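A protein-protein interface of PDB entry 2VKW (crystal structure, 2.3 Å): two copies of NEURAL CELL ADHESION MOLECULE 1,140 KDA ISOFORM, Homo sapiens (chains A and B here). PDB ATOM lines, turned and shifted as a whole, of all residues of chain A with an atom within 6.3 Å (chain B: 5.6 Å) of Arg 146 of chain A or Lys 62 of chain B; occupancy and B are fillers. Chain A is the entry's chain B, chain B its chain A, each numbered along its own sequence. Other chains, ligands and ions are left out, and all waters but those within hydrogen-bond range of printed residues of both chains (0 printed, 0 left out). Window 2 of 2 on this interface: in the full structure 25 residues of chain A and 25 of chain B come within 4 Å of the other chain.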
ATOM      1  N   LEU A 144     -13.283  -9.553   8.784  1.00  0.00           N
ATOM      2  CA  LEU A 144     -14.268 -10.139   7.881  1.00  0.00           C
ATOM      3  C   LEU A 144     -15.572 -10.250   8.668  1.00  0.00           C
ATOM      4  O   LEU A 144     -15.595 -10.809   9.764  1.00  0.00           O
ATOM      5  CB  LEU A 144     -13.797 -11.521   7.427  1.00  0.00           C
ATOM      6  CG  LEU A 144     -12.339 -11.605   6.954  1.00  0.00           C
ATOM      7  CD1 LEU A 144     -12.014 -13.038   6.557  1.00  0.00           C
ATOM      8  CD2 LEU A 144     -12.113 -10.680   5.783  1.00  0.00           C
ATOM      9  N   VAL A 145     -16.651  -9.712   8.113  1.00  0.00           N
ATOM     10  CA  VAL A 145     -17.933  -9.723   8.806  1.00  0.00           C
ATOM     11  C   VAL A 145     -19.048 -10.393   8.018  1.00  0.00           C
ATOM     12  O   VAL A 145     -19.300 -10.054   6.865  1.00  0.00           O
ATOM     13  CB  VAL A 145     -18.361  -8.270   9.173  1.00  0.00           C
ATOM     14  CG1 VAL A 145     -19.675  -8.269   9.921  1.00  0.00           C
ATOM     15  CG2 VAL A 145     -17.275  -7.618  10.030  1.00  0.00           C
ATOM     16  N   ARG A 146     -19.687 -11.368   8.656  1.00  0.00           N
ATOM     17  CA  ARG A 146     -20.806 -12.105   8.083  1.00  0.00           C
ATOM     18  C   ARG A 146     -21.990 -11.928   9.020  1.00  0.00           C
ATOM     19  O   ARG A 146     -21.838 -12.028  10.241  1.00  0.00           O
ATOM     20  CB  ARG A 146     -20.484 -13.595   7.993  1.00  0.00           C
ATOM     21  CG  ARG A 146     -19.599 -13.982   6.840  1.00  0.00           C
ATOM     22  CD  ARG A 146     -20.338 -13.766   5.536  1.00  0.00           C
ATOM     23  NE  ARG A 146     -19.594 -14.273   4.392  1.00  0.00           N
ATOM     24  CZ  ARG A 146     -20.143 -14.513   3.208  1.00  0.00           C
ATOM     25  NH1 ARG A 146     -21.440 -14.288   3.027  1.00  0.00           N
ATOM     26  NH2 ARG A 146     -19.402 -14.986   2.217  1.00  0.00           N
ATOM     27  N   TYR A 147     -23.167 -11.663   8.462  1.00  0.00           N
ATOM     28  CA  TYR A 147     -24.358 -11.514   9.287  1.00  0.00           C
ATOM     29  C   TYR A 147     -25.623 -11.826   8.497  1.00  0.00           C
ATOM     30  O   TYR A 147     -25.622 -11.832   7.259  1.00  0.00           O
ATOM     31  CB  TYR A 147     -24.420 -10.110   9.896  1.00  0.00           C
ATOM     32  CG  TYR A 147     -24.921  -9.033   8.975  1.00  0.00           C
ATOM     33  CD1 TYR A 147     -26.250  -8.633   9.006  1.00  0.00           C
ATOM     34  CD2 TYR A 147     -24.074  -8.420   8.065  1.00  0.00           C
ATOM     35  CE1 TYR A 147     -26.721  -7.648   8.155  1.00  0.00           C
ATOM     36  CE2 TYR A 147     -24.537  -7.434   7.203  1.00  0.00           C
ATOM     37  CZ  TYR A 147     -25.860  -7.055   7.255  1.00  0.00           C
ATOM     38  OH  TYR A 147     -26.332  -6.088   6.399  1.00  0.00           O
ATOM     39  N   ARG A 148     -26.701 -12.082   9.224  1.00  0.00           N
ATOM     40  CA  ARG A 148     -27.974 -12.438   8.615  1.00  0.00           C
ATOM     41  C   ARG A 148     -29.039 -12.336   9.688  1.00  0.00           C
ATOM     42  O   ARG A 148     -28.733 -12.246  10.873  1.00  0.00           O
ATOM     43  CB  ARG A 148     -27.939 -13.902   8.181  1.00  0.00           C
ATOM     44  CG  ARG A 148     -27.928 -14.819   9.424  1.00  0.00           C
ATOM     45  CD  ARG A 148     -27.666 -16.305   9.172  1.00  0.00           C
ATOM     46  NE  ARG A 148     -28.817 -17.017   8.638  1.00  0.00           N
ATOM     47  CZ  ARG A 148     -29.158 -18.259   8.972  1.00  0.00           C
ATOM     48  NH1 ARG A 148     -28.447 -18.949   9.854  1.00  0.00           N
ATOM     49  NH2 ARG A 148     -30.210 -18.822   8.402  1.00  0.00           N
ATOM     50  N   GLU A 153     -31.411 -15.488   4.496  1.00  0.00           N
ATOM     51  CA  GLU A 153     -30.096 -15.799   3.952  1.00  0.00           C
ATOM     52  C   GLU A 153     -28.998 -14.841   4.395  1.00  0.00           C
ATOM     53  O   GLU A 153     -29.268 -13.709   4.791  1.00  0.00           O
ATOM     54  CB  GLU A 153     -30.184 -15.825   2.422  1.00  0.00           C
ATOM     55  CG  GLU A 153     -28.912 -16.250   1.720  1.00  0.00           C
ATOM     56  CD  GLU A 153     -28.445 -17.632   2.142  1.00  0.00           C
ATOM     57  OE1 GLU A 153     -29.192 -18.603   1.910  1.00  0.00           O
ATOM     58  OE2 GLU A 153     -27.328 -17.744   2.705  1.00  0.00           O
ATOM     59  N   TRP A 154     -27.754 -15.305   4.320  1.00  0.00           N
ATOM     60  CA  TRP A 154     -26.617 -14.482   4.707  1.00  0.00           C
ATOM     61  C   TRP A 154     -26.453 -13.306   3.761  1.00  0.00           C
ATOM     62  O   TRP A 154     -26.748 -13.412   2.569  1.00  0.00           O
ATOM     63  CB  TRP A 154     -25.325 -15.298   4.689  1.00  0.00           C
ATOM     64  CG  TRP A 154     -25.262 -16.358   5.726  1.00  0.00           C
ATOM     65  CD1 TRP A 154     -25.589 -17.668   5.571  1.00  0.00           C
ATOM     66  CD2 TRP A 154     -24.874 -16.197   7.096  1.00  0.00           C
ATOM     67  NE1 TRP A 154     -25.428 -18.342   6.757  1.00  0.00           N
ATOM     68  CE2 TRP A 154     -24.992 -17.463   7.712  1.00  0.00           C
ATOM     69  CE3 TRP A 154     -24.441 -15.108   7.864  1.00  0.00           C
ATOM     70  CZ2 TRP A 154     -24.694 -17.673   9.060  1.00  0.00           C
ATOM     71  CZ3 TRP A 154     -24.144 -15.314   9.212  1.00  0.00           C
ATOM     72  CH2 TRP A 154     -24.272 -16.588   9.794  1.00  0.00           C
ATOM     73  N   LYS A 155     -25.990 -12.184   4.300  1.00  0.00           N
ATOM     74  CA  LYS A 155     -25.736 -10.992   3.497  1.00  0.00           C
ATOM     75  C   LYS A 155     -24.303 -11.129   2.991  1.00  0.00           C
ATOM     76  O   LYS A 155     -23.523 -11.923   3.530  1.00  0.00           O
ATOM     77  CB  LYS A 155     -25.862  -9.731   4.358  1.00  0.00           C
ATOM     78  CG  LYS A 155     -27.224  -9.582   5.034  1.00  0.00           C
ATOM     79  CD  LYS A 155     -28.294  -9.150   4.050  1.00  0.00           C
ATOM     80  CE  LYS A 155     -27.980  -7.761   3.514  1.00  0.00           C
ATOM     81  NZ  LYS A 155     -29.105  -7.166   2.735  1.00  0.00           N
ATOM     82  N   PRO A 156     -23.932 -10.369   1.949  1.00  0.00           N
ATOM     83  CA  PRO A 156     -22.559 -10.487   1.452  1.00  0.00           C
ATOM     84  C   PRO A 156     -21.567 -10.136   2.554  1.00  0.00           C
ATOM     85  O   PRO A 156     -21.893  -9.386   3.475  1.00  0.00           O
ATOM     86  CB  PRO A 156     -22.524  -9.490   0.298  1.00  0.00           C
ATOM     87  CG  PRO A 156     -23.949  -9.508  -0.205  1.00  0.00           C
ATOM     88  CD  PRO A 156     -24.725  -9.468   1.099  1.00  0.00           C
ATOM     89  N   GLU A 157     -20.363 -10.689   2.459  1.00  0.00           N
ATOM     90  CA  GLU A 157     -19.320 -10.435   3.439  1.00  0.00           C
ATOM     91  C   GLU A 157     -18.874  -8.977   3.440  1.00  0.00           C
ATOM     92  O   GLU A 157     -18.752  -8.357   2.380  1.00  0.00           O
ATOM     93  CB  GLU A 157     -18.108 -11.325   3.156  1.00  0.00           C
ATOM     94  CG  GLU A 157     -16.932 -11.070   4.075  1.00  0.00           C
ATOM     95  CD  GLU A 157     -15.718 -11.906   3.724  1.00  0.00           C
ATOM     96  OE1 GLU A 157     -15.131 -11.686   2.643  1.00  0.00           O
ATOM     97  OE2 GLU A 157     -15.351 -12.787   4.533  1.00  0.00           O
ATOM     98  N   ILE A 158     -18.632  -8.440   4.633  1.00  0.00           N
ATOM     99  CA  ILE A 158     -18.164  -7.065   4.803  1.00  0.00           C
ATOM    100  C   ILE A 158     -16.697  -7.100   5.238  1.00  0.00           C
ATOM    101  O   ILE A 158     -16.349  -7.763   6.222  1.00  0.00           O
ATOM    102  CB  ILE A 158     -18.940  -6.312   5.919  1.00  0.00           C
ATOM    103  CG1 ILE A 158     -20.444  -6.425   5.697  1.00  0.00           C
ATOM    104  CG2 ILE A 158     -18.515  -4.849   5.945  1.00  0.00           C
ATOM    105  CD1 ILE A 158     -21.272  -5.811   6.822  1.00  0.00           C
ATOM    106  N   GLU A 179     -27.718 -12.672  13.780  1.00  0.00           N
ATOM    107  CA  GLU A 179     -26.502 -13.283  14.279  1.00  0.00           C
ATOM    108  C   GLU A 179     -25.355 -12.675  13.473  1.00  0.00           C
ATOM    109  O   GLU A 179     -25.501 -12.406  12.278  1.00  0.00           O
ATOM    110  CB  GLU A 179     -26.552 -14.801  14.127  1.00  0.00           C
ATOM    111  CG  GLU A 179     -26.392 -15.333  12.727  1.00  0.00           C
ATOM    112  CD  GLU A 179     -26.467 -16.846  12.694  1.00  0.00           C
ATOM    113  OE1 GLU A 179     -25.917 -17.486  13.616  1.00  0.00           O
ATOM    114  OE2 GLU A 179     -27.064 -17.399  11.747  1.00  0.00           O
ATOM    115  N   VAL A 180     -24.226 -12.442  14.135  1.00  0.00           N
ATOM    116  CA  VAL A 180     -23.064 -11.849  13.484  1.00  0.00           C
ATOM    117  C   VAL A 180     -21.777 -12.610  13.791  1.00  0.00           C
ATOM    118  O   VAL A 180     -21.571 -13.064  14.920  1.00  0.00           O
ATOM    119  CB  VAL A 180     -22.873 -10.381  13.942  1.00  0.00           C
ATOM    120  CG1 VAL A 180     -21.732  -9.730  13.177  1.00  0.00           C
ATOM    121  CG2 VAL A 180     -24.154  -9.610  13.732  1.00  0.00           C
ATOM    122  N   TYR A 181     -20.912 -12.735  12.785  1.00  0.00           N
ATOM    123  CA  TYR A 181     -19.621 -13.409  12.938  1.00  0.00           C
ATOM    124  C   TYR A 181     -18.526 -12.468  12.444  1.00  0.00           C
ATOM    125  O   TYR A 181     -18.651 -11.849  11.385  1.00  0.00           O
ATOM    126  CB  TYR A 181     -19.585 -14.716  12.135  1.00  0.00           C
ATOM    127  CG  TYR A 181     -20.342 -15.846  12.779  1.00  0.00           C
ATOM    128  CD1 TYR A 181     -19.728 -16.675  13.717  1.00  0.00           C
ATOM    129  CD2 TYR A 181     -21.683 -16.062  12.490  1.00  0.00           C
ATOM    130  CE1 TYR A 181     -20.435 -17.687  14.355  1.00  0.00           C
ATOM    131  CE2 TYR A 181     -22.403 -17.066  13.120  1.00  0.00           C
ATOM    132  CZ  TYR A 181     -21.775 -17.875  14.054  1.00  0.00           C
ATOM    133  OH  TYR A 181     -22.490 -18.847  14.705  1.00  0.00           O
ATOM    134  N   VAL A 182     -17.459 -12.355  13.222  1.00  0.00           N
ATOM    135  CA  VAL A 182     -16.361 -11.478  12.860  1.00  0.00           C
ATOM    136  C   VAL A 182     -15.025 -12.186  12.984  1.00  0.00           C
ATOM    137  O   VAL A 182     -14.678 -12.717  14.041  1.00  0.00           O
ATOM    138  CB  VAL A 182     -16.319 -10.238  13.751  1.00  0.00           C
ATOM    139  CG1 VAL A 182     -15.265  -9.261  13.227  1.00  0.00           C
ATOM    140  CG2 VAL A 182     -17.676  -9.598  13.806  1.00  0.00           C
ATOM    141  N   ILE B  39     -21.993 -26.051  -0.243  1.00  0.00           N
ATOM    142  CA  ILE B  39     -22.840 -26.799   0.671  1.00  0.00           C
ATOM    143  C   ILE B  39     -23.756 -25.774   1.345  1.00  0.00           C
ATOM    144  O   ILE B  39     -23.294 -24.737   1.820  1.00  0.00           O
ATOM    145  CB  ILE B  39     -21.988 -27.506   1.729  1.00  0.00           C
ATOM    146  CG1 ILE B  39     -21.100 -28.555   1.055  1.00  0.00           C
ATOM    147  CG2 ILE B  39     -22.881 -28.143   2.772  1.00  0.00           C
ATOM    148  CD1 ILE B  39     -20.032 -29.110   1.961  1.00  0.00           C
ATOM    149  N   LEU B  40     -25.051 -26.063   1.384  1.00  0.00           N
ATOM    150  CA  LEU B  40     -26.020 -25.144   1.978  1.00  0.00           C
ATOM    151  C   LEU B  40     -26.393 -25.476   3.420  1.00  0.00           C
ATOM    152  O   LEU B  40     -26.538 -24.576   4.251  1.00  0.00           O
ATOM    153  CB  LEU B  40     -27.286 -25.108   1.129  1.00  0.00           C
ATOM    154  CG  LEU B  40     -27.090 -24.805  -0.359  1.00  0.00           C
ATOM    155  CD1 LEU B  40     -28.432 -24.811  -1.059  1.00  0.00           C
ATOM    156  CD2 LEU B  40     -26.406 -23.452  -0.525  1.00  0.00           C
ATOM    157  N   ASP B  60     -27.603 -24.736   9.396  1.00  0.00           N
ATOM    158  CA  ASP B  60     -27.023 -23.873   8.385  1.00  0.00           C
ATOM    159  C   ASP B  60     -25.532 -24.187   8.230  1.00  0.00           C
ATOM    160  O   ASP B  60     -24.799 -24.280   9.217  1.00  0.00           O
ATOM    161  CB  ASP B  60     -27.210 -22.413   8.774  1.00  0.00           C
ATOM    162  CG  ASP B  60     -26.743 -21.479   7.696  1.00  0.00           C
ATOM    163  OD1 ASP B  60     -27.352 -21.502   6.608  1.00  0.00           O
ATOM    164  OD2 ASP B  60     -25.767 -20.744   7.934  1.00  0.00           O
ATOM    165  N   ALA B  61     -25.091 -24.344   6.985  1.00  0.00           N
ATOM    166  CA  ALA B  61     -23.701 -24.667   6.702  1.00  0.00           C
ATOM    167  C   ALA B  61     -22.715 -23.588   7.158  1.00  0.00           C
ATOM    168  O   ALA B  61     -21.876 -23.842   8.023  1.00  0.00           O
ATOM    169  CB  ALA B  61     -23.536 -24.948   5.216  1.00  0.00           C
ATOM    170  N   LYS B  62     -22.812 -22.392   6.587  1.00  0.00           N
ATOM    171  CA  LYS B  62     -21.903 -21.303   6.958  1.00  0.00           C
ATOM    172  C   LYS B  62     -21.800 -21.144   8.473  1.00  0.00           C
ATOM    173  O   LYS B  62     -20.708 -21.019   9.028  1.00  0.00           O
ATOM    174  CB  LYS B  62     -22.356 -19.974   6.338  1.00  0.00           C
ATOM    175  CG  LYS B  62     -21.422 -18.809   6.688  1.00  0.00           C
ATOM    176  CD  LYS B  62     -21.878 -17.476   6.091  1.00  0.00           C
ATOM    177  CE  LYS B  62     -21.280 -17.217   4.718  1.00  0.00           C
ATOM    178  NZ  LYS B  62     -21.635 -18.251   3.718  1.00  0.00           N
ATOM    179  N   GLU B  63     -22.950 -21.151   9.132  1.00  0.00           N
ATOM    180  CA  GLU B  63     -23.018 -21.021  10.577  1.00  0.00           C
ATOM    181  C   GLU B  63     -22.192 -22.133  11.225  1.00  0.00           C
ATOM    182  O   GLU B  63     -21.305 -21.871  12.044  1.00  0.00           O
ATOM    183  CB  GLU B  63     -24.483 -21.118  11.018  1.00  0.00           C
ATOM    184  CG  GLU B  63     -24.751 -20.791  12.472  1.00  0.00           C
ATOM    185  CD  GLU B  63     -26.234 -20.862  12.813  1.00  0.00           C
ATOM    186  OE1 GLU B  63     -26.783 -21.984  12.893  1.00  0.00           O
ATOM    187  OE2 GLU B  63     -26.851 -19.792  12.992  1.00  0.00           O
ATOM    188  N   ALA B  64     -22.480 -23.373  10.839  1.00  0.00           N
ATOM    189  CA  ALA B  64     -21.777 -24.534  11.378  1.00  0.00           C
ATOM    190  C   ALA B  64     -20.282 -24.495  11.080  1.00  0.00           C
ATOM    191  O   ALA B  64     -19.463 -24.865  11.913  1.00  0.00           O
ATOM    192  CB  ALA B  64     -22.385 -25.818  10.814  1.00  0.00           C
ATOM    193  N   SER B  65     -19.928 -24.049   9.884  1.00  0.00           N
ATOM    194  CA  SER B  65     -18.526 -23.975   9.503  1.00  0.00           C
ATOM    195  C   SER B  65     -17.727 -23.030  10.398  1.00  0.00           C
ATOM    196  O   SER B  65     -16.604 -23.336  10.789  1.00  0.00           O
ATOM    197  CB  SER B  65     -18.402 -23.519   8.049  1.00  0.00           C
ATOM    198  OG  SER B  65     -17.044 -23.329   7.696  1.00  0.00           O
ATOM    199  N   MET B  66     -18.316 -21.886  10.722  1.00  0.00           N
ATOM    200  CA  MET B  66     -17.646 -20.893  11.548  1.00  0.00           C
ATOM    201  C   MET B  66     -17.451 -21.323  12.999  1.00  0.00           C
ATOM    202  O   MET B  66     -16.542 -20.836  13.676  1.00  0.00           O
ATOM    203  CB  MET B  66     -18.406 -19.561  11.474  1.00  0.00           C
ATOM    204  CG  MET B  66     -18.532 -19.056  10.040  1.00  0.00           C
ATOM    205  SD  MET B  66     -19.183 -17.385   9.811  1.00  0.00           S
ATOM    206  CE  MET B  66     -17.641 -16.462   9.832  1.00  0.00           C
ATOM    207  N   GLU B  67     -18.285 -22.243  13.476  1.00  0.00           N
ATOM    208  CA  GLU B  67     -18.161 -22.710  14.851  1.00  0.00           C
ATOM    209  C   GLU B  67     -17.509 -24.084  14.925  1.00  0.00           C
ATOM    210  O   GLU B  67     -17.048 -24.493  15.984  1.00  0.00           O
ATOM    211  CB  GLU B  67     -19.530 -22.754  15.522  1.00  0.00           C
ATOM    212  CG  GLU B  67     -20.248 -21.430  15.484  1.00  0.00           C
ATOM    213  CD  GLU B  67     -21.591 -21.479  16.167  1.00  0.00           C
ATOM    214  OE1 GLU B  67     -22.295 -22.502  16.002  1.00  0.00           O
ATOM    215  OE2 GLU B  67     -21.947 -20.494  16.855  1.00  0.00           O
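Printed residues of chain A that touch a printed residue of chain B: Arg 146, Arg 148, Trp 154, Glu 179 and Tyr 181. Hydrophobic or aromatic side chains of chain A within 4 Å of the printed part of chain B: Trp 154 and Tyr 181. Of the 10 printed residues of chain B, 5 touch a printed residue of chain A. Printed residues of chain B that touch a printed residue of chain A: Asp 60, Lys 62, Glu 63, Met 66 and Glu 67. Hydrophobic or aromatic side chains of chain B within 4 Å of the printed part of chain A: Met 66. Among the printed residues, 10 pairs touch across the chains. Among the printed residues, Asp or Glu carboxylates within 4 Å of a Lys or Arg side-chain nitrogen of the other chain: Arg 148 of chain A with Asp 60 of chain B (3.8 Å) and Arg 148 of chain A with Glu 63 of chain B (3.6 Å).
The guanidinium group of Arg 148 of chain A lies within salt-bridge range of the side-chain carboxylate of Glu 179 of chain A (2.8 Å). The guanidinium group (NH1) of Arg 146 of chain A lies within hydrogen-bond range of the backbone carbonyl oxygen (O) of Lys 155 of chain A (3.2 Å). The backbone NH (N) of Glu 63 of chain B sits at hydrogen-bond distance from the side-chain carboxylate (OD2) of Asp 60 of chain B (3.1 Å). The backbone NH (N) of Tyr 181 of chain A lies within hydrogen-bond range of the backbone carbonyl oxygen (O) of Arg 146 of chain A, 2.8 Å away.
Among the printed residues, pairs that only touch across the chains: Arg 146 of chain A with Lys 62 of chain B (3.3 Å), Trp 154 of chain A with Lys 62 of chain B (3.4 Å), Tyr 181 of chain A with Met 66 of chain B (3.5 Å), Tyr 181 of chain A with Glu 63 of chain B (3.7 Å) and Trp 154 of chain A with Glu 63 of chain B (3.9 Å).
No position is printed for both chains. Of the 10 pairs that touch across the chains among the printed residues, none has its exchanged pair printed and touching as well.
Tyr 147 of chain A touches none of the printed residues of chain B. Of the printed residues of chain B, Arg 148 of chain A touches Asp 60 and Glu 63. Printed residues of chain B within 4 Å of Trp 154 of chain A: Asp 60, Lys 62 and Glu 63. Printed residues of chain B within 4 Å of Glu 179 of chain A: Glu 63 (2.6 Å). Printed residues of chain B within 4 Å of Tyr 181 of chain A: Glu 63 (3.7 Å), Met 66 (3.5 Å) and Glu 67 (2.8 Å). Of the printed residues of chain A, Asp 60 of chain B touches Arg 148 and Trp 154. Of chain A, only Arg 146 and Trp 154 come within 4 Å of Lys 62 of chain B. The nearest residue of chain A that does not touch Lys 62 of chain B is Glu 153 of chain A (5.8 Å).
The side-chain carboxylate (OD2) of Asp 60 of chain B lies within hydrogen-bond range of the indole nitrogen (NE1) of Trp 154 of chain A. The side-chain hydroxyl of Tyr 181 of chain A is in hydrogen-bond range of the side-chain carboxylate of Glu 67 of chain B, 2.8 Å away. OE1 of Glu 179 of chain A sits close to OE2 of Glu 63 of chain B. The side-chain carboxylate of Asp 60 of chain B lies within salt-bridge range of the guanidinium group of Arg 148 of chain A (3.8 Å). OE2 of Glu 63 of chain B lies within salt-bridge range of NH1 of Arg 148 of chain A (3.6 Å).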
